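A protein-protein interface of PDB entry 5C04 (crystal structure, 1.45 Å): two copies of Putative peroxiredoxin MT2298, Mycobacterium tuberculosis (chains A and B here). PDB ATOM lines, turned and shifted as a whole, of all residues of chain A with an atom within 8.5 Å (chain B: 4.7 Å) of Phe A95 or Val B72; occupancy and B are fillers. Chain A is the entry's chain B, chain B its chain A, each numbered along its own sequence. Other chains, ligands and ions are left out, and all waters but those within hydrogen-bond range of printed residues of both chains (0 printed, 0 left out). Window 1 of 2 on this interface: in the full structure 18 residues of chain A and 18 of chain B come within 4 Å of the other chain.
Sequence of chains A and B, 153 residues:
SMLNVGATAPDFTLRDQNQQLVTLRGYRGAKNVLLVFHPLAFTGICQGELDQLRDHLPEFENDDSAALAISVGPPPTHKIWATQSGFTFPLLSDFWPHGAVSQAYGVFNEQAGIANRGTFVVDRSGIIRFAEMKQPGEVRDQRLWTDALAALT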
ATOM      1  N   LEU A  14      -2.760   4.877  -2.316  1.00  0.00           N
ATOM      2  CA  LEU A  14      -1.350   5.047  -2.106  1.00  0.00           C
ATOM      3  C   LEU A  14      -0.534   4.520  -3.284  1.00  0.00           C
ATOM      4  O   LEU A  14      -0.989   3.644  -4.012  1.00  0.00           O
ATOM      5  CB  LEU A  14      -0.865   4.316  -0.860  1.00  0.00           C
ATOM      6  CG  LEU A  14      -1.461   4.772   0.497  1.00  0.00           C
ATOM      7  CD1 LEU A  14      -0.987   3.896   1.640  1.00  0.00           C
ATOM      8  CD2 LEU A  14      -1.076   6.217   0.774  1.00  0.00           C
ATOM      9  N   ARG A  15       0.659   5.053  -3.453  1.00  0.00           N
ATOM     10  CA  ARG A  15       1.589   4.579  -4.506  1.00  0.00           C
ATOM     11  C   ARG A  15       2.311   3.332  -4.051  1.00  0.00           C
ATOM     12  O   ARG A  15       2.815   3.270  -2.934  1.00  0.00           O
ATOM     13  CB  ARG A  15       2.638   5.630  -4.819  1.00  0.00           C
ATOM     14  CG  ARG A  15       2.083   6.964  -5.287  1.00  0.00           C
ATOM     15  CD  ARG A  15       2.008   7.062  -6.800  1.00  0.00           C
ATOM     16  NE  ARG A  15       1.306   8.278  -7.217  1.00  0.00           N
ATOM     17  CZ  ARG A  15       0.820   8.478  -8.440  1.00  0.00           C
ATOM     18  NH1 ARG A  15       0.968   7.553  -9.382  1.00  0.00           N
ATOM     19  NH2 ARG A  15       0.173   9.610  -8.719  1.00  0.00           N
ATOM     20  N   GLN A  19       5.225   3.083  -8.382  1.00  0.00           N
ATOM     21  CA  GLN A  19       4.484   4.359  -8.433  1.00  0.00           C
ATOM     22  C   GLN A  19       3.100   4.257  -8.998  1.00  0.00           C
ATOM     23  O   GLN A  19       2.503   5.248  -9.436  1.00  0.00           O
ATOM     24  CB  GLN A  19       5.265   5.409  -9.217  1.00  0.00           C
ATOM     25  CG  GLN A  19       6.581   5.740  -8.577  1.00  0.00           C
ATOM     26  CD  GLN A  19       6.626   7.159  -8.137  1.00  0.00           C
ATOM     27  OE1 GLN A  19       7.362   7.962  -8.725  1.00  0.00           O
ATOM     28  NE2 GLN A  19       5.812   7.506  -7.152  1.00  0.00           N
ATOM     29  N   LEU A  40       9.851   0.104   9.054  1.00  0.00           N
ATOM     30  CA  LEU A  40      10.822   0.655   8.088  1.00  0.00           C
ATOM     31  C   LEU A  40      11.503  -0.386   7.232  1.00  0.00           C
ATOM     32  O   LEU A  40      12.058  -1.382   7.728  1.00  0.00           O
ATOM     33  CB  LEU A  40      11.942   1.404   8.811  1.00  0.00           C
ATOM     34  CG  LEU A  40      11.683   2.764   9.453  1.00  0.00           C
ATOM     35  CD1 LEU A  40      12.915   3.300  10.161  1.00  0.00           C
ATOM     36  CD2 LEU A  40      11.176   3.758   8.449  1.00  0.00           C
ATOM     37  N   ILE A  70       2.327  -1.794   4.137  1.00  0.00           N
ATOM     38  CA  ILE A  70       2.254  -0.324   4.212  1.00  0.00           C
ATOM     39  C   ILE A  70       3.272   0.194   5.212  1.00  0.00           C
ATOM     40  O   ILE A  70       3.362  -0.280   6.345  1.00  0.00           O
ATOM     41  CB  ILE A  70       0.845   0.154   4.663  1.00  0.00           C
ATOM     42  CG1 ILE A  70      -0.230  -0.398   3.724  1.00  0.00           C
ATOM     43  CG2 ILE A  70       0.780   1.683   4.733  1.00  0.00           C
ATOM     44  CD1 ILE A  70      -1.682  -0.158   4.091  1.00  0.00           C
ATOM     45  N   SER A  71       4.059   1.187   4.787  1.00  0.00           N
ATOM     46  CA  SER A  71       5.086   1.806   5.611  1.00  0.00           C
ATOM     47  C   SER A  71       5.260   3.266   5.155  1.00  0.00           C
ATOM     48  O   SER A  71       4.849   3.625   4.049  1.00  0.00           O
ATOM     49  CB  SER A  71       6.389   1.027   5.456  1.00  0.00           C
ATOM     50  OG  SER A  71       7.321   1.367   6.446  1.00  0.00           O
ATOM     51  N   VAL A  72       5.941   4.056   5.971  1.00  0.00           N
ATOM     52  CA  VAL A  72       6.158   5.469   5.657  1.00  0.00           C
ATOM     53  C   VAL A  72       7.227   5.759   4.604  1.00  0.00           C
ATOM     54  O   VAL A  72       7.391   6.920   4.227  1.00  0.00           O
ATOM     55  CB  VAL A  72       6.452   6.293   6.936  1.00  0.00           C
ATOM     56  CG1 VAL A  72       5.287   6.200   7.907  1.00  0.00           C
ATOM     57  CG2 VAL A  72       7.761   5.898   7.597  1.00  0.00           C
ATOM     58  N   GLY A  73       7.918   4.757   4.071  1.00  0.00           N
ATOM     59  CA  GLY A  73       8.906   5.010   3.056  1.00  0.00           C
ATOM     60  C   GLY A  73       8.310   5.358   1.705  1.00  0.00           C
ATOM     61  O   GLY A  73       7.179   4.963   1.387  1.00  0.00           O
ATOM     62  N   PRO A  74       9.035   6.142   0.892  1.00  0.00           N
ATOM     63  CA  PRO A  74       8.582   6.510  -0.448  1.00  0.00           C
ATOM     64  C   PRO A  74       8.853   5.381  -1.468  1.00  0.00           C
ATOM     65  O   PRO A  74       9.599   4.454  -1.197  1.00  0.00           O
ATOM     66  CB  PRO A  74       9.432   7.737  -0.764  1.00  0.00           C
ATOM     67  CG  PRO A  74      10.714   7.436  -0.056  1.00  0.00           C
ATOM     68  CD  PRO A  74      10.338   6.739   1.210  1.00  0.00           C
ATOM     69  N   PRO A  75       8.230   5.467  -2.640  1.00  0.00           N
ATOM     70  CA  PRO A  75       8.378   4.358  -3.581  1.00  0.00           C
ATOM     71  C   PRO A  75       9.782   3.955  -3.954  1.00  0.00           C
ATOM     72  O   PRO A  75      10.048   2.759  -4.059  1.00  0.00           O
ATOM     73  CB  PRO A  75       7.484   4.776  -4.747  1.00  0.00           C
ATOM     74  CG  PRO A  75       6.447   5.653  -4.135  1.00  0.00           C
ATOM     75  CD  PRO A  75       7.219   6.433  -3.103  1.00  0.00           C
ATOM     76  N   PRO A  76      10.732   4.883  -4.149  1.00  0.00           N
ATOM     77  CA  PRO A  76      12.067   4.397  -4.544  1.00  0.00           C
ATOM     78  C   PRO A  76      12.726   3.499  -3.499  1.00  0.00           C
ATOM     79  O   PRO A  76      13.472   2.584  -3.841  1.00  0.00           O
ATOM     80  CB  PRO A  76      12.871   5.703  -4.761  1.00  0.00           C
ATOM     81  CG  PRO A  76      11.807   6.714  -5.084  1.00  0.00           C
ATOM     82  CD  PRO A  76      10.612   6.349  -4.267  1.00  0.00           C
ATOM     83  N   THR A  77      12.497   3.795  -2.215  1.00  0.00           N
ATOM     84  CA  THR A  77      13.004   2.943  -1.147  1.00  0.00           C
ATOM     85  C   THR A  77      12.384   1.567  -1.229  1.00  0.00           C
ATOM     86  O   THR A  77      13.085   0.536  -1.144  1.00  0.00           O
ATOM     87  CB  THR A  77      12.705   3.574   0.228  1.00  0.00           C
ATOM     88  OG1 THR A  77      13.497   4.752   0.357  1.00  0.00           O
ATOM     89  CG2 THR A  77      13.027   2.653   1.419  1.00  0.00           C
ATOM     90  N   HIS A  78      11.064   1.553  -1.341  1.00  0.00           N
ATOM     91  CA  HIS A  78      10.331   0.280  -1.441  1.00  0.00           C
ATOM     92  C   HIS A  78      10.708  -0.505  -2.692  1.00  0.00           C
ATOM     93  O   HIS A  78      10.767  -1.736  -2.675  1.00  0.00           O
ATOM     94  CB  HIS A  78       8.858   0.494  -1.292  1.00  0.00           C
ATOM     95  CG  HIS A  78       8.466   0.939   0.091  1.00  0.00           C
ATOM     96  ND1 HIS A  78       7.273   1.545   0.373  1.00  0.00           N
ATOM     97  CD2 HIS A  78       9.164   0.901   1.255  1.00  0.00           C
ATOM     98  CE1 HIS A  78       7.216   1.805   1.667  1.00  0.00           C
ATOM     99  NE2 HIS A  78       8.368   1.466   2.217  1.00  0.00           N
ATOM    100  N   LEU A  92       3.247  -0.296  -0.155  1.00  0.00           N
ATOM    101  CA  LEU A  92       2.608   1.011  -0.349  1.00  0.00           C
ATOM    102  C   LEU A  92       3.238   2.065   0.533  1.00  0.00           C
ATOM    103  O   LEU A  92       3.631   1.811   1.681  1.00  0.00           O
ATOM    104  CB  LEU A  92       1.121   0.930  -0.007  1.00  0.00           C
ATOM    105  CG  LEU A  92       0.317  -0.147  -0.740  1.00  0.00           C
ATOM    106  CD1 LEU A  92      -1.166   0.019  -0.409  1.00  0.00           C
ATOM    107  CD2 LEU A  92       0.558  -0.085  -2.236  1.00  0.00           C
ATOM    108  N   SER A  93       3.310   3.263  -0.030  1.00  0.00           N
ATOM    109  CA  SER A  93       3.996   4.389   0.616  1.00  0.00           C
ATOM    110  C   SER A  93       3.036   5.339   1.383  1.00  0.00           C
ATOM    111  O   SER A  93       2.302   6.080   0.746  1.00  0.00           O
ATOM    112  CB  SER A  93       4.731   5.183  -0.441  1.00  0.00           C
ATOM    113  OG  SER A  93       5.871   4.487  -0.908  1.00  0.00           O
ATOM    114  N   ASP A  94       3.088   5.313   2.702  1.00  0.00           N
ATOM    115  CA  ASP A  94       2.319   6.217   3.554  1.00  0.00           C
ATOM    116  C   ASP A  94       3.239   7.410   3.883  1.00  0.00           C
ATOM    117  O   ASP A  94       3.532   7.691   5.044  1.00  0.00           O
ATOM    118  CB  ASP A  94       1.846   5.443   4.800  1.00  0.00           C
ATOM    119  CG  ASP A  94       0.781   6.176   5.620  1.00  0.00           C
ATOM    120  OD1 ASP A  94       0.099   7.062   5.076  1.00  0.00           O
ATOM    121  OD2 ASP A  94       0.638   5.801   6.796  1.00  0.00           O
ATOM    122  N   PHE A  95       3.731   8.082   2.831  1.00  0.00           N
ATOM    123  CA  PHE A  95       4.936   8.922   2.872  1.00  0.00           C
ATOM    124  C   PHE A  95       4.648  10.418   3.011  1.00  0.00           C
ATOM    125  O   PHE A  95       5.329  11.114   3.781  1.00  0.00           O
ATOM    126  CB  PHE A  95       5.781   8.660   1.614  1.00  0.00           C
ATOM    127  CG  PHE A  95       6.895   9.636   1.408  1.00  0.00           C
ATOM    128  CD1 PHE A  95       8.055   9.513   2.144  1.00  0.00           C
ATOM    129  CD2 PHE A  95       6.819  10.619   0.439  1.00  0.00           C
ATOM    130  CE1 PHE A  95       9.101  10.382   1.976  1.00  0.00           C
ATOM    131  CE2 PHE A  95       7.843  11.529   0.268  1.00  0.00           C
ATOM    132  CZ  PHE A  95       8.997  11.389   1.027  1.00  0.00           C
ATOM    133  N   TRP A  96       3.677  10.917   2.258  1.00  0.00           N
ATOM    134  CA  TRP A  96       3.362  12.369   2.267  1.00  0.00           C
ATOM    135  C   TRP A  96       1.914  12.542   1.800  1.00  0.00           C
ATOM    136  O   TRP A  96       1.627  12.385   0.606  1.00  0.00           O
ATOM    137  CB  TRP A  96       4.356  13.116   1.383  1.00  0.00           C
ATOM    138  CG  TRP A  96       4.277  14.623   1.528  1.00  0.00           C
ATOM    139  CD1 TRP A  96       3.877  15.540   0.578  1.00  0.00           C
ATOM    140  CD2 TRP A  96       4.649  15.369   2.676  1.00  0.00           C
ATOM    141  NE1 TRP A  96       3.960  16.813   1.092  1.00  0.00           N
ATOM    142  CE2 TRP A  96       4.431  16.738   2.378  1.00  0.00           C
ATOM    143  CE3 TRP A  96       5.147  15.024   3.936  1.00  0.00           C
ATOM    144  CZ2 TRP A  96       4.717  17.750   3.294  1.00  0.00           C
ATOM    145  CZ3 TRP A  96       5.421  16.045   4.857  1.00  0.00           C
ATOM    146  CH2 TRP A  96       5.194  17.384   4.529  1.00  0.00           C
ATOM    147  N   PRO A  97       0.997  12.846   2.709  1.00  0.00           N
ATOM    148  CA  PRO A  97       1.229  13.095   4.137  1.00  0.00           C
ATOM    149  C   PRO A  97       1.781  11.906   4.932  1.00  0.00           C
ATOM    150  O   PRO A  97       1.326  10.763   4.765  1.00  0.00           O
ATOM    151  CB  PRO A  97      -0.176  13.479   4.641  1.00  0.00           C
ATOM    152  CG  PRO A  97      -1.103  12.799   3.700  1.00  0.00           C
ATOM    153  CD  PRO A  97      -0.435  12.870   2.370  1.00  0.00           C
ATOM    154  N   HIS A  98       2.714  12.188   5.823  1.00  0.00           N
ATOM    155  CA  HIS A  98       3.528  11.178   6.487  1.00  0.00           C
ATOM    156  C   HIS A  98       2.735  10.459   7.540  1.00  0.00           C
ATOM    157  O   HIS A  98       2.315  11.057   8.544  1.00  0.00           O
ATOM    158  CB  HIS A  98       4.734  11.906   7.099  1.00  0.00           C
ATOM    159  CG  HIS A  98       5.752  11.045   7.780  1.00  0.00           C
ATOM    160  ND1 HIS A  98       7.111  11.206   7.570  1.00  0.00           N
ATOM    161  CD2 HIS A  98       5.641  10.048   8.682  1.00  0.00           C
ATOM    162  CE1 HIS A  98       7.784  10.355   8.317  1.00  0.00           C
ATOM    163  NE2 HIS A  98       6.912   9.631   8.997  1.00  0.00           N
ATOM    164  N   GLY A  99       2.488   9.164   7.312  1.00  0.00           N
ATOM    165  CA  GLY A  99       1.773   8.371   8.311  1.00  0.00           C
ATOM    166  C   GLY A  99       0.280   8.585   8.336  1.00  0.00           C
ATOM    167  O   GLY A  99      -0.357   8.096   9.254  1.00  0.00           O
ATOM    168  N   ALA A 100      -0.303   9.239   7.326  1.00  0.00           N
ATOM    169  CA  ALA A 100      -1.753   9.532   7.379  1.00  0.00           C
ATOM    170  C   ALA A 100      -2.627   8.299   7.418  1.00  0.00           C
ATOM    171  O   ALA A 100      -3.595   8.222   8.177  1.00  0.00           O
ATOM    172  CB  ALA A 100      -2.180  10.381   6.196  1.00  0.00           C
ATOM    173  N   VAL A 101      -2.309   7.301   6.594  1.00  0.00           N
ATOM    174  CA  VAL A 101      -3.093   6.083   6.605  1.00  0.00           C
ATOM    175  C   VAL A 101      -2.881   5.298   7.908  1.00  0.00           C
ATOM    176  O   VAL A 101      -3.849   4.793   8.494  1.00  0.00           O
ATOM    177  CB  VAL A 101      -2.792   5.224   5.352  1.00  0.00           C
ATOM    178  CG1 VAL A 101      -3.595   3.942   5.371  1.00  0.00           C
ATOM    179  CG2 VAL A 101      -3.151   6.019   4.107  1.00  0.00           C
ATOM    180  N   SER A 102      -1.638   5.208   8.368  1.00  0.00           N
ATOM    181  CA  SER A 102      -1.319   4.543   9.627  1.00  0.00           C
ATOM    182  C   SER A 102      -2.113   5.211  10.760  1.00  0.00           C
ATOM    183  O   SER A 102      -2.665   4.503  11.640  1.00  0.00           O
ATOM    184  CB  SER A 102       0.175   4.635   9.912  1.00  0.00           C
ATOM    185  OG  SER A 102       0.955   3.989   8.905  1.00  0.00           O
ATOM    186  N   GLY A 113       7.560   8.508  14.400  1.00  0.00           N
ATOM    187  CA  GLY A 113       7.246   8.803  12.995  1.00  0.00           C
ATOM    188  C   GLY A 113       7.146   7.585  12.083  1.00  0.00           C
ATOM    189  O   GLY A 113       7.333   7.691  10.859  1.00  0.00           O
ATOM    190  N   PRO B  39      16.609  15.387  -2.786  1.00  0.00           N
ATOM    191  CA  PRO B  39      15.333  14.691  -2.695  1.00  0.00           C
ATOM    192  C   PRO B  39      15.283  13.299  -2.037  1.00  0.00           C
ATOM    193  O   PRO B  39      14.639  13.146  -0.992  1.00  0.00           O
ATOM    194  CB  PRO B  39      14.890  14.625  -4.160  1.00  0.00           C
ATOM    195  CG  PRO B  39      15.400  15.878  -4.745  1.00  0.00           C
ATOM    196  CD  PRO B  39      16.719  16.146  -4.040  1.00  0.00           C
ATOM    197  N   LEU B  40      15.909  12.282  -2.626  1.00  0.00           N
ATOM    198  CA  LEU B  40      15.639  10.919  -2.201  1.00  0.00           C
ATOM    199  C   LEU B  40      16.746   9.946  -2.538  1.00  0.00           C
ATOM    200  O   LEU B  40      17.198   9.860  -3.691  1.00  0.00           O
ATOM    201  CB  LEU B  40      14.371  10.378  -2.865  1.00  0.00           C
ATOM    202  CG  LEU B  40      12.989  10.873  -2.387  1.00  0.00           C
ATOM    203  CD1 LEU B  40      11.892  10.279  -3.276  1.00  0.00           C
ATOM    204  CD2 LEU B  40      12.775  10.549  -0.919  1.00  0.00           C
ATOM    205  N   SER B  71      18.621  14.584   3.633  1.00  0.00           N
ATOM    206  CA  SER B  71      17.437  14.174   2.896  1.00  0.00           C
ATOM    207  C   SER B  71      16.407  13.684   3.897  1.00  0.00           C
ATOM    208  O   SER B  71      16.762  13.411   5.041  1.00  0.00           O
ATOM    209  CB  SER B  71      17.816  13.071   1.923  1.00  0.00           C
ATOM    210  OG  SER B  71      16.799  12.888   0.954  1.00  0.00           O
ATOM    211  N   VAL B  72      15.156  13.525   3.439  1.00  0.00           N
ATOM    212  CA  VAL B  72      14.080  13.091   4.338  1.00  0.00           C
ATOM    213  C   VAL B  72      14.088  11.603   4.698  1.00  0.00           C
ATOM    214  O   VAL B  72      13.252  11.189   5.514  1.00  0.00           O
ATOM    215  CB  VAL B  72      12.687  13.520   3.807  1.00  0.00           C
ATOM    216  CG1 VAL B  72      12.563  15.038   3.724  1.00  0.00           C
ATOM    217  CG2 VAL B  72      12.342  12.824   2.505  1.00  0.00           C
ATOM    218  N   GLY B  73      15.012  10.792   4.175  1.00  0.00           N
ATOM    219  CA  GLY B  73      15.046   9.385   4.518  1.00  0.00           C
ATOM    220  C   GLY B  73      15.564   9.124   5.913  1.00  0.00           C
ATOM    221  O   GLY B  73      16.372   9.901   6.415  1.00  0.00           O
ATOM    222  N   PRO B  74      15.135   8.031   6.538  1.00  0.00           N
ATOM    223  CA  PRO B  74      15.635   7.628   7.831  1.00  0.00           C
ATOM    224  C   PRO B  74      16.983   6.915   7.738  1.00  0.00           C
ATOM    225  O   PRO B  74      17.392   6.481   6.661  1.00  0.00           O
ATOM    226  CB  PRO B  74      14.542   6.708   8.343  1.00  0.00           C
ATOM    227  CG  PRO B  74      14.021   6.056   7.113  1.00  0.00           C
ATOM    228  CD  PRO B  74      14.131   7.087   6.015  1.00  0.00           C
ATOM    229  N   ASP B  94      16.529  13.981   7.756  1.00  0.00           N
ATOM    230  CA  ASP B  94      15.559  15.030   8.062  1.00  0.00           C
ATOM    231  C   ASP B  94      14.147  14.384   8.044  1.00  0.00           C
ATOM    232  O   ASP B  94      13.248  14.811   7.327  1.00  0.00           O
ATOM    233  CB  ASP B  94      15.714  16.173   7.028  1.00  0.00           C
ATOM    234  CG  ASP B  94      14.985  17.457   7.429  1.00  0.00           C
ATOM    235  OD1 ASP B  94      14.661  17.662   8.635  1.00  0.00           O
ATOM    236  OD2 ASP B  94      14.704  18.274   6.523  1.00  0.00           O
ATOM    237  N   PHE B  95      14.002  13.365   8.887  1.00  0.00           N
ATOM    238  CA  PHE B  95      12.944  12.347   8.749  1.00  0.00           C
ATOM    239  C   PHE B  95      11.686  12.589   9.586  1.00  0.00           C
ATOM    240  O   PHE B  95      10.561  12.429   9.088  1.00  0.00           O
ATOM    241  CB  PHE B  95      13.526  10.994   9.122  1.00  0.00           C
ATOM    242  CG  PHE B  95      12.502   9.891   9.259  1.00  0.00           C
ATOM    243  CD1 PHE B  95      11.969   9.295   8.126  1.00  0.00           C
ATOM    244  CD2 PHE B  95      12.123   9.428  10.509  1.00  0.00           C
ATOM    245  CE1 PHE B  95      11.033   8.294   8.230  1.00  0.00           C
ATOM    246  CE2 PHE B  95      11.184   8.437  10.624  1.00  0.00           C
ATOM    247  CZ  PHE B  95      10.651   7.872   9.487  1.00  0.00           C
ATOM    248  N   HIS B  98       9.231  15.629   9.654  1.00  0.00           N
ATOM    249  CA  HIS B  98       9.505  15.379   8.225  1.00  0.00           C
ATOM    250  C   HIS B  98       9.878  16.687   7.496  1.00  0.00           C
ATOM    251  O   HIS B  98       9.050  17.577   7.326  1.00  0.00           O
ATOM    252  CB  HIS B  98       8.258  14.744   7.610  1.00  0.00           C
ATOM    253  CG  HIS B  98       8.396  14.304   6.181  1.00  0.00           C
ATOM    254  ND1 HIS B  98       7.981  13.068   5.734  1.00  0.00           N
ATOM    255  CD2 HIS B  98       8.814  14.969   5.077  1.00  0.00           C
ATOM    256  CE1 HIS B  98       8.148  12.979   4.432  1.00  0.00           C
ATOM    257  NE2 HIS B  98       8.674  14.119   4.011  1.00  0.00           N
ATOM    258  N   GLY B  99      11.140  16.793   7.058  1.00  0.00           N
ATOM    259  CA  GLY B  99      11.565  17.980   6.352  1.00  0.00           C
ATOM    260  C   GLY B  99      11.767  19.243   7.187  1.00  0.00           C
ATOM    261  O   GLY B  99      11.850  20.324   6.606  1.00  0.00           O
ATOM    262  N   PHE B 108      12.523  23.235   1.269  1.00  0.00           N
ATOM    263  CA  PHE B 108      11.618  22.079   1.279  1.00  0.00           C
ATOM    264  C   PHE B 108      10.588  22.250   0.170  1.00  0.00           C
ATOM    265  O   PHE B 108      10.059  23.374  -0.044  1.00  0.00           O
ATOM    266  CB  PHE B 108      10.963  21.945   2.646  1.00  0.00           C
ATOM    267  CG  PHE B 108      10.139  20.690   2.828  1.00  0.00           C
ATOM    268  CD1 PHE B 108      10.727  19.430   2.802  1.00  0.00           C
ATOM    269  CD2 PHE B 108       8.775  20.783   3.081  1.00  0.00           C
ATOM    270  CE1 PHE B 108       9.948  18.291   3.032  1.00  0.00           C
ATOM    271  CE2 PHE B 108       8.001  19.642   3.294  1.00  0.00           C
ATOM    272  CZ  PHE B 108       8.596  18.407   3.239  1.00  0.00           C
ATOM    273  N   ALA B 112       5.669  17.889  -2.778  1.00  0.00           N
ATOM    274  CA  ALA B 112       6.202  16.550  -2.948  1.00  0.00           C
ATOM    275  C   ALA B 112       6.704  15.889  -1.657  1.00  0.00           C
ATOM    276  O   ALA B 112       6.859  14.670  -1.621  1.00  0.00           O
ATOM    277  CB  ALA B 112       7.288  16.567  -3.994  1.00  0.00           C
ATOM    278  N   GLY B 113       6.921  16.655  -0.594  1.00  0.00           N
ATOM    279  CA  GLY B 113       7.389  16.102   0.677  1.00  0.00           C
ATOM    280  C   GLY B 113       8.869  15.754   0.708  1.00  0.00           C
ATOM    281  O   GLY B 113       9.321  14.927   1.521  1.00  0.00           O
ATOM    282  N   ILE B 114       9.644  16.419  -0.130  1.00  0.00           N
ATOM    283  CA  ILE B 114      11.076  16.190  -0.216  1.00  0.00           C
ATOM    284  C   ILE B 114      11.821  17.518  -0.192  1.00  0.00           C
ATOM    285  O   ILE B 114      11.263  18.557  -0.540  1.00  0.00           O
ATOM    286  CB  ILE B 114      11.432  15.432  -1.520  1.00  0.00           C
ATOM    287  CG1 ILE B 114      10.907  16.211  -2.748  1.00  0.00           C
ATOM    288  CG2 ILE B 114      10.944  14.000  -1.467  1.00  0.00           C
ATOM    289  CD1 ILE B 114      11.178  15.594  -4.093  1.00  0.00           C
ATOM    290  N   ALA B 115      13.102  17.474   0.150  1.00  0.00           N
ATOM    291  CA  ALA B 115      13.954  18.649  -0.052  1.00  0.00           C
ATOM    292  C   ALA B 115      14.179  18.825  -1.541  1.00  0.00           C
ATOM    293  O   ALA B 115      14.343  17.840  -2.291  1.00  0.00           O
ATOM    294  CB  ALA B 115      15.275  18.495   0.678  1.00  0.00           C
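ND1 of His B98 lies within hydrogen-bond range of ND1 of His A98, at 2.8 Å.
NE1 of Trp A96 lies close to N of Gly B113.
NE2 of His B98 sits at hydrogen-bond distance from O of Gly B113 (2.7 Å).
A ring nitrogen (NE2) of His A98 lies within hydrogen-bond range of the backbone carbonyl oxygen (O) of Gly A113 (2.7 Å).
Among the printed residues, pairs that only touch across the chains: Leu A40 with Pro B74, Val A72 with Phe B95, Pro A74 with Leu B40, Pro A76 with Leu B40, Phe A95 with Val B72, Phe A95 with His B98, Phe A95 with Ala B112, Phe A95 with Gly B113, Trp A96 with His B98, Trp A96 with Phe B108, Trp A96 with Ala B112, His A98 with Phe B95 and Gly A113 with Phe B95.
Pro A97 touches none of the printed residues of chain B.
Printed residues of chain B within 4 Å of His A98: Phe B95 (3.6 Å) and His B98 (2.8 Å).
Of the printed residues of chain A, Val B72 touches Phe A95 (3.9 Å).
No residue of chain A comes within 4 Å of Gly B73.
Of the printed residues of chain A, Ala B112 touches Phe A95 (3.8 Å) and Trp A96 (3.6 Å).
Of the printed residues of chain A, Gly B113 touches Phe A95 and Trp A96.
The nearest residue of chain B that does not touch Phe A95 is Ile B114 (4.1 Å).
The nearest printed residue of chain A that does not touch His B98 is Val A72 (6.1 Å).
Among the printed residues, no Asp or Glu carboxylate lies within 4 Å of a Lys or Arg side-chain nitrogen of the other chain.
Leu A40 touches Pro B74, and with the chains exchanged Pro A74 touches Leu B40.
Phe A95 touches His B98, and with the chains exchanged His A98 touches Phe B95.
Phe A95 touches Gly B113, and with the chains exchanged Gly A113 touches Phe B95.
His B98 touches its own counterpart, His A98.
10 positions are printed for both chains.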
